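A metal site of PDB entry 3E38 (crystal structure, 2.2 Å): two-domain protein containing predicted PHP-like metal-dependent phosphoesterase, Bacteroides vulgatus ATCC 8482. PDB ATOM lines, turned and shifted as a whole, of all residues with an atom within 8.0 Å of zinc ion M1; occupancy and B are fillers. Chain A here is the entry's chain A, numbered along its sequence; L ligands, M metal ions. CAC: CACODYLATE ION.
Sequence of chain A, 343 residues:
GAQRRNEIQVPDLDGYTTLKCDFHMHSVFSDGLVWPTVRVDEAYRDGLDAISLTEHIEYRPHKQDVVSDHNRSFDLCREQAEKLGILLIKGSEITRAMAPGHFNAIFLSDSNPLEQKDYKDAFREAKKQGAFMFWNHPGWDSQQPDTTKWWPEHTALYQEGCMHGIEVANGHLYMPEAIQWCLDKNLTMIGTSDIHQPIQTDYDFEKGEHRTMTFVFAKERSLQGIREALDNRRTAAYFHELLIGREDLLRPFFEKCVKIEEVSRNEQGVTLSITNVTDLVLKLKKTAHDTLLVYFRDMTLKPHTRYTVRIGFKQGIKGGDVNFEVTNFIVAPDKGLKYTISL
The backbone carbonyl oxygen (O) of Thr 54 sits close to a ring nitrogen (ND1) of His 26 (3.3 Å).
A ring nitrogen (ND1) of His 26 is in hydrogen-bond range of the side-chain hydroxyl (OG) of Ser 30 (3.1 Å).
A ring nitrogen (ND1) of His 56 lies within hydrogen-bond range of the side-chain hydroxyl (OG1) of Thr 95 (2.6 Å).
ND1 of His 196 lies within hydrogen-bond range of O of Asp 194 (2.8 Å).
The backbone NH (N) of His 56 lies close to the side-chain hydroxyl (OG) of Ser 30, at 3.5 Å.
A ring nitrogen (ND1) of His 56 sits close to the side-chain carboxylate (OE1) of Glu 93, at 3.3 Å.
The backbone NH (N) of His 26 lies within hydrogen-bond range of the backbone carbonyl oxygen (O) of Ile 195 (2.9 Å).
Zinc ion M1 is bound by NE2 of His 196, OD2 of Asp 31, NE2 of His 56 and OD1 of Asp 31.
Zinc ion M1 has four donor atoms within binding distance.
Slightly farther from zinc ion M1 lies O1 of the ligand (2.6 Å).
Residues that only touch zinc ion M1: His 26.
Four residues have an atom within 4 Å of zinc ion M1: His 26, Asp 31, His 56 and His 196.
The nearest printed residue that does not touch zinc ion M1 is Tyr 59 (4.8 Å).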
ATOM      1  N   HIS A  24     -12.456 -19.300 -30.628  1.00  0.00           N
ATOM      2  CA  HIS A  24     -11.769 -18.680 -29.473  1.00  0.00           C
ATOM      3  C   HIS A  24     -12.428 -17.388 -29.088  1.00  0.00           C
ATOM      4  O   HIS A  24     -12.420 -16.429 -29.824  1.00  0.00           O
ATOM      5  CB  HIS A  24     -10.339 -18.380 -29.881  1.00  0.00           C
ATOM      6  CG  HIS A  24      -9.391 -18.097 -28.765  1.00  0.00           C
ATOM      7  ND1 HIS A  24      -8.027 -18.218 -28.925  1.00  0.00           N
ATOM      8  CD2 HIS A  24      -9.581 -17.697 -27.487  1.00  0.00           C
ATOM      9  CE1 HIS A  24      -7.417 -17.881 -27.806  1.00  0.00           C
ATOM     10  NE2 HIS A  24      -8.334 -17.561 -26.918  1.00  0.00           N
ATOM     11  N   MET A  25     -13.008 -17.345 -27.917  1.00  0.00           N
ATOM     12  CA  MET A  25     -13.669 -16.122 -27.506  1.00  0.00           C
ATOM     13  C   MET A  25     -14.037 -16.180 -26.050  1.00  0.00           C
ATOM     14  O   MET A  25     -14.080 -17.283 -25.439  1.00  0.00           O
ATOM     15  CB  MET A  25     -14.897 -15.893 -28.395  1.00  0.00           C
ATOM     16  CG  MET A  25     -16.124 -16.742 -28.059  1.00  0.00           C
ATOM     17  SD  MET A  25     -17.380 -16.512 -29.533  1.00  0.00           S
ATOM     18  CE  MET A  25     -16.053 -16.777 -30.927  1.00  0.00           C
ATOM     19  N   HIS A  26     -14.299 -14.993 -25.508  1.00  0.00           N
ATOM     20  CA  HIS A  26     -14.564 -14.871 -24.067  1.00  0.00           C
ATOM     21  C   HIS A  26     -15.764 -14.053 -23.682  1.00  0.00           C
ATOM     22  O   HIS A  26     -16.266 -13.244 -24.434  1.00  0.00           O
ATOM     23  CB  HIS A  26     -13.323 -14.286 -23.375  1.00  0.00           C
ATOM     24  CG  HIS A  26     -12.075 -15.062 -23.635  1.00  0.00           C
ATOM     25  ND1 HIS A  26     -11.613 -16.037 -22.779  1.00  0.00           N
ATOM     26  CD2 HIS A  26     -11.201 -15.002 -24.660  1.00  0.00           C
ATOM     27  CE1 HIS A  26     -10.497 -16.559 -23.278  1.00  0.00           C
ATOM     28  NE2 HIS A  26     -10.232 -15.938 -24.421  1.00  0.00           N
ATOM     29  N   SER A  27     -16.240 -14.335 -22.473  1.00  0.00           N
ATOM     30  CA  SER A  27     -17.380 -13.612 -21.881  1.00  0.00           C
ATOM     31  C   SER A  27     -17.023 -13.294 -20.455  1.00  0.00           C
ATOM     32  O   SER A  27     -15.910 -13.572 -20.021  1.00  0.00           O
ATOM     33  CB  SER A  27     -18.658 -14.441 -21.845  1.00  0.00           C
ATOM     34  OG  SER A  27     -18.583 -15.543 -20.909  1.00  0.00           O
ATOM     35  N   SER A  30     -15.238 -15.573 -17.856  1.00  0.00           N
ATOM     36  CA  SER A  30     -13.757 -15.530 -17.705  1.00  0.00           C
ATOM     37  C   SER A  30     -13.369 -14.044 -17.672  1.00  0.00           C
ATOM     38  O   SER A  30     -13.808 -13.306 -16.766  1.00  0.00           O
ATOM     39  CB  SER A  30     -12.957 -16.346 -18.753  1.00  0.00           C
ATOM     40  OG  SER A  30     -13.199 -16.002 -20.107  1.00  0.00           O
ATOM     41  N   ASP A  31     -12.580 -13.595 -18.645  1.00  0.00           N
ATOM     42  CA  ASP A  31     -12.161 -12.187 -18.700  1.00  0.00           C
ATOM     43  C   ASP A  31     -12.768 -11.401 -19.842  1.00  0.00           C
ATOM     44  O   ASP A  31     -12.317 -10.326 -20.151  1.00  0.00           O
ATOM     45  CB  ASP A  31     -10.643 -12.005 -18.734  1.00  0.00           C
ATOM     46  CG  ASP A  31     -10.036 -12.536 -20.002  1.00  0.00           C
ATOM     47  OD1 ASP A  31     -10.723 -13.228 -20.773  1.00  0.00           O
ATOM     48  OD2 ASP A  31      -8.847 -12.267 -20.208  1.00  0.00           O
ATOM     49  N   GLY A  32     -13.794 -11.942 -20.460  1.00  0.00           N
ATOM     50  CA  GLY A  32     -14.541 -11.207 -21.462  1.00  0.00           C
ATOM     51  C   GLY A  32     -15.456 -10.194 -20.810  1.00  0.00           C
ATOM     52  O   GLY A  32     -15.607 -10.163 -19.590  1.00  0.00           O
ATOM     53  N   THR A  54     -14.703 -20.067 -25.295  1.00  0.00           N
ATOM     54  CA  THR A  54     -13.606 -20.744 -24.632  1.00  0.00           C
ATOM     55  C   THR A  54     -13.052 -19.914 -23.479  1.00  0.00           C
ATOM     56  O   THR A  54     -12.006 -19.244 -23.605  1.00  0.00           O
ATOM     57  CB  THR A  54     -12.511 -21.048 -25.679  1.00  0.00           C
ATOM     58  OG1 THR A  54     -11.992 -19.815 -26.227  1.00  0.00           O
ATOM     59  CG2 THR A  54     -13.136 -21.896 -26.760  1.00  0.00           C
ATOM     60  N   GLU A  55     -13.781 -19.972 -22.365  1.00  0.00           N
ATOM     61  CA  GLU A  55     -13.410 -19.227 -21.182  1.00  0.00           C
ATOM     62  C   GLU A  55     -12.041 -19.744 -20.658  1.00  0.00           C
ATOM     63  O   GLU A  55     -11.698 -20.918 -20.797  1.00  0.00           O
ATOM     64  CB  GLU A  55     -14.440 -19.356 -20.073  1.00  0.00           C
ATOM     65  CG  GLU A  55     -15.937 -19.183 -20.391  1.00  0.00           C
ATOM     66  CD  GLU A  55     -16.346 -17.844 -21.018  1.00  0.00           C
ATOM     67  OE1 GLU A  55     -15.544 -16.898 -21.115  1.00  0.00           O
ATOM     68  OE2 GLU A  55     -17.538 -17.767 -21.363  1.00  0.00           O
ATOM     69  N   HIS A  56     -11.248 -18.880 -20.065  1.00  0.00           N
ATOM     70  CA  HIS A  56     -10.029 -19.364 -19.407  1.00  0.00           C
ATOM     71  C   HIS A  56     -10.454 -20.250 -18.255  1.00  0.00           C
ATOM     72  O   HIS A  56     -11.457 -20.005 -17.581  1.00  0.00           O
ATOM     73  CB  HIS A  56      -9.156 -18.272 -18.822  1.00  0.00           C
ATOM     74  CG  HIS A  56      -8.741 -17.214 -19.787  1.00  0.00           C
ATOM     75  ND1 HIS A  56      -7.560 -17.276 -20.494  1.00  0.00           N
ATOM     76  CD2 HIS A  56      -9.347 -16.061 -20.147  1.00  0.00           C
ATOM     77  CE1 HIS A  56      -7.461 -16.195 -21.246  1.00  0.00           C
ATOM     78  NE2 HIS A  56      -8.551 -15.451 -21.077  1.00  0.00           N
ATOM     79  N   TYR A  59      -7.992 -18.278 -15.287  1.00  0.00           N
ATOM     80  CA  TYR A  59      -8.127 -16.833 -15.143  1.00  0.00           C
ATOM     81  C   TYR A  59      -9.550 -16.387 -15.287  1.00  0.00           C
ATOM     82  O   TYR A  59     -10.046 -16.228 -16.401  1.00  0.00           O
ATOM     83  CB  TYR A  59      -7.269 -16.101 -16.197  1.00  0.00           C
ATOM     84  CG  TYR A  59      -7.262 -14.577 -16.052  1.00  0.00           C
ATOM     85  CD1 TYR A  59      -6.838 -13.996 -14.873  1.00  0.00           C
ATOM     86  CD2 TYR A  59      -7.626 -13.736 -17.111  1.00  0.00           C
ATOM     87  CE1 TYR A  59      -6.829 -12.639 -14.702  1.00  0.00           C
ATOM     88  CE2 TYR A  59      -7.580 -12.336 -16.952  1.00  0.00           C
ATOM     89  CZ  TYR A  59      -7.182 -11.810 -15.735  1.00  0.00           C
ATOM     90  OH  TYR A  59      -7.103 -10.471 -15.483  1.00  0.00           O
ATOM     91  N   PRO A  61     -11.255 -13.371 -13.528  1.00  0.00           N
ATOM     92  CA  PRO A  61     -11.131 -12.223 -12.656  1.00  0.00           C
ATOM     93  C   PRO A  61     -12.451 -11.666 -12.159  1.00  0.00           C
ATOM     94  O   PRO A  61     -12.463 -10.799 -11.291  1.00  0.00           O
ATOM     95  CB  PRO A  61     -10.404 -11.186 -13.525  1.00  0.00           C
ATOM     96  CG  PRO A  61     -10.585 -11.600 -14.906  1.00  0.00           C
ATOM     97  CD  PRO A  61     -10.911 -13.046 -14.924  1.00  0.00           C
ATOM     98  N   GLU A  93     -10.124 -22.440 -22.582  1.00  0.00           N
ATOM     99  CA  GLU A  93      -8.739 -22.058 -22.731  1.00  0.00           C
ATOM    100  C   GLU A  93      -7.819 -22.387 -21.531  1.00  0.00           C
ATOM    101  O   GLU A  93      -7.957 -21.848 -20.489  1.00  0.00           O
ATOM    102  CB  GLU A  93      -8.648 -20.574 -23.049  1.00  0.00           C
ATOM    103  CG  GLU A  93      -7.219 -20.183 -23.278  1.00  0.00           C
ATOM    104  CD  GLU A  93      -7.056 -18.774 -23.775  1.00  0.00           C
ATOM    105  OE1 GLU A  93      -8.015 -17.954 -23.731  1.00  0.00           O
ATOM    106  OE2 GLU A  93      -5.946 -18.518 -24.231  1.00  0.00           O
ATOM    107  N   THR A  95      -4.775 -21.799 -19.739  1.00  0.00           N
ATOM    108  CA  THR A  95      -4.049 -20.525 -19.648  1.00  0.00           C
ATOM    109  C   THR A  95      -2.906 -20.617 -18.681  1.00  0.00           C
ATOM    110  O   THR A  95      -3.068 -20.574 -17.487  1.00  0.00           O
ATOM    111  CB  THR A  95      -5.025 -19.413 -19.157  1.00  0.00           C
ATOM    112  OG1 THR A  95      -6.261 -19.483 -19.884  1.00  0.00           O
ATOM    113  CG2 THR A  95      -4.443 -18.024 -19.299  1.00  0.00           C
ATOM    114  N   HIS A 102      -0.599 -20.693 -23.829  1.00  0.00           N
ATOM    115  CA  HIS A 102      -2.058 -20.903 -23.828  1.00  0.00           C
ATOM    116  C   HIS A 102      -2.534 -21.802 -24.937  1.00  0.00           C
ATOM    117  O   HIS A 102      -2.170 -21.581 -26.084  1.00  0.00           O
ATOM    118  CB  HIS A 102      -2.769 -19.575 -24.061  1.00  0.00           C
ATOM    119  CG  HIS A 102      -2.522 -18.541 -23.021  1.00  0.00           C
ATOM    120  ND1 HIS A 102      -3.344 -17.454 -22.859  1.00  0.00           N
ATOM    121  CD2 HIS A 102      -1.535 -18.411 -22.088  1.00  0.00           C
ATOM    122  CE1 HIS A 102      -2.907 -16.714 -21.865  1.00  0.00           C
ATOM    123  NE2 HIS A 102      -1.799 -17.261 -21.394  1.00  0.00           N
ATOM    124  N   HIS A 137      -2.261 -17.987 -30.001  1.00  0.00           N
ATOM    125  CA  HIS A 137      -1.412 -16.811 -30.118  1.00  0.00           C
ATOM    126  C   HIS A 137       0.055 -17.079 -29.751  1.00  0.00           C
ATOM    127  O   HIS A 137       0.610 -16.438 -28.856  1.00  0.00           O
ATOM    128  CB  HIS A 137      -1.960 -15.629 -29.240  1.00  0.00           C
ATOM    129  CG  HIS A 137      -2.328 -15.994 -27.825  1.00  0.00           C
ATOM    130  ND1 HIS A 137      -1.383 -16.307 -26.857  1.00  0.00           N
ATOM    131  CD2 HIS A 137      -3.537 -16.050 -27.200  1.00  0.00           C
ATOM    132  CE1 HIS A 137      -1.999 -16.581 -25.719  1.00  0.00           C
ATOM    133  NE2 HIS A 137      -3.309 -16.461 -25.900  1.00  0.00           N
ATOM    134  N   TRP A 140       2.049 -13.839 -29.363  1.00  0.00           N
ATOM    135  CA  TRP A 140       1.622 -12.817 -28.410  1.00  0.00           C
ATOM    136  C   TRP A 140       2.861 -12.280 -27.679  1.00  0.00           C
ATOM    137  O   TRP A 140       3.566 -13.037 -27.019  1.00  0.00           O
ATOM    138  CB  TRP A 140       0.631 -13.393 -27.424  1.00  0.00           C
ATOM    139  CG  TRP A 140       0.061 -12.440 -26.512  1.00  0.00           C
ATOM    140  CD1 TRP A 140      -0.261 -11.112 -26.772  1.00  0.00           C
ATOM    141  CD2 TRP A 140      -0.366 -12.704 -25.176  1.00  0.00           C
ATOM    142  NE1 TRP A 140      -0.830 -10.537 -25.647  1.00  0.00           N
ATOM    143  CE2 TRP A 140      -0.907 -11.497 -24.658  1.00  0.00           C
ATOM    144  CE3 TRP A 140      -0.330 -13.830 -24.355  1.00  0.00           C
ATOM    145  CZ2 TRP A 140      -1.406 -11.410 -23.362  1.00  0.00           C
ATOM    146  CZ3 TRP A 140      -0.831 -13.748 -23.067  1.00  0.00           C
ATOM    147  CH2 TRP A 140      -1.368 -12.542 -22.587  1.00  0.00           C
ATOM    148  N   ASP A 194     -10.512 -14.255 -30.544  1.00  0.00           N
ATOM    149  CA  ASP A 194     -10.143 -14.125 -29.119  1.00  0.00           C
ATOM    150  C   ASP A 194     -10.830 -12.888 -28.563  1.00  0.00           C
ATOM    151  O   ASP A 194     -10.298 -12.136 -27.754  1.00  0.00           O
ATOM    152  CB  ASP A 194      -8.637 -14.009 -28.993  1.00  0.00           C
ATOM    153  CG  ASP A 194      -8.106 -14.358 -27.589  1.00  0.00           C
ATOM    154  OD1 ASP A 194      -8.914 -14.466 -26.646  1.00  0.00           O
ATOM    155  OD2 ASP A 194      -6.865 -14.577 -27.461  1.00  0.00           O
ATOM    156  N   ILE A 195     -12.036 -12.639 -29.030  1.00  0.00           N
ATOM    157  CA  ILE A 195     -12.801 -11.441 -28.591  1.00  0.00           C
ATOM    158  C   ILE A 195     -13.096 -11.413 -27.101  1.00  0.00           C
ATOM    159  O   ILE A 195     -13.582 -12.357 -26.527  1.00  0.00           O
ATOM    160  CB  ILE A 195     -14.108 -11.252 -29.465  1.00  0.00           C
ATOM    161  CG1 ILE A 195     -14.743  -9.850 -29.278  1.00  0.00           C
ATOM    162  CG2 ILE A 195     -15.114 -12.366 -29.190  1.00  0.00           C
ATOM    163  CD1 ILE A 195     -13.820  -8.654 -29.732  1.00  0.00           C
ATOM    164  N   HIS A 196     -12.744 -10.310 -26.458  1.00  0.00           N
ATOM    165  CA  HIS A 196     -13.082 -10.061 -25.045  1.00  0.00           C
ATOM    166  C   HIS A 196     -14.109  -8.908 -24.973  1.00  0.00           C
ATOM    167  O   HIS A 196     -15.020  -8.938 -24.187  1.00  0.00           O
ATOM    168  CB  HIS A 196     -11.848  -9.698 -24.186  1.00  0.00           C
ATOM    169  CG  HIS A 196     -10.840 -10.812 -23.997  1.00  0.00           C
ATOM    170  ND1 HIS A 196     -10.137 -11.354 -25.046  1.00  0.00           N
ATOM    171  CD2 HIS A 196     -10.379 -11.409 -22.877  1.00  0.00           C
ATOM    172  CE1 HIS A 196      -9.282 -12.256 -24.579  1.00  0.00           C
ATOM    173  NE2 HIS A 196      -9.417 -12.303 -23.264  1.00  0.00           N
HETATM  174 AS   CAC L   1      -6.184 -13.878 -23.474  1.00  0.00          AS
HETATM  175  O1  CAC L   1      -7.559 -14.860 -23.930  1.00  0.00           O
HETATM  176  O2  CAC L   1      -4.741 -14.842 -23.266  1.00  0.00           O
HETATM  177  C1  CAC L   1      -5.829 -12.728 -25.049  1.00  0.00           C
HETATM  178  C2  CAC L   1      -6.408 -12.951 -21.771  1.00  0.00           C
HETATM  179 ZN    ZN M   1      -8.463 -13.488 -21.874  1.00  0.00          ZN
HETATM  180 ZN    ZN M   2      -8.332 -16.162 -25.061  1.00  0.00          ZN
HETATM  181 ZN    ZN M   3      -4.833 -16.607 -24.359  1.00  0.00          ZN
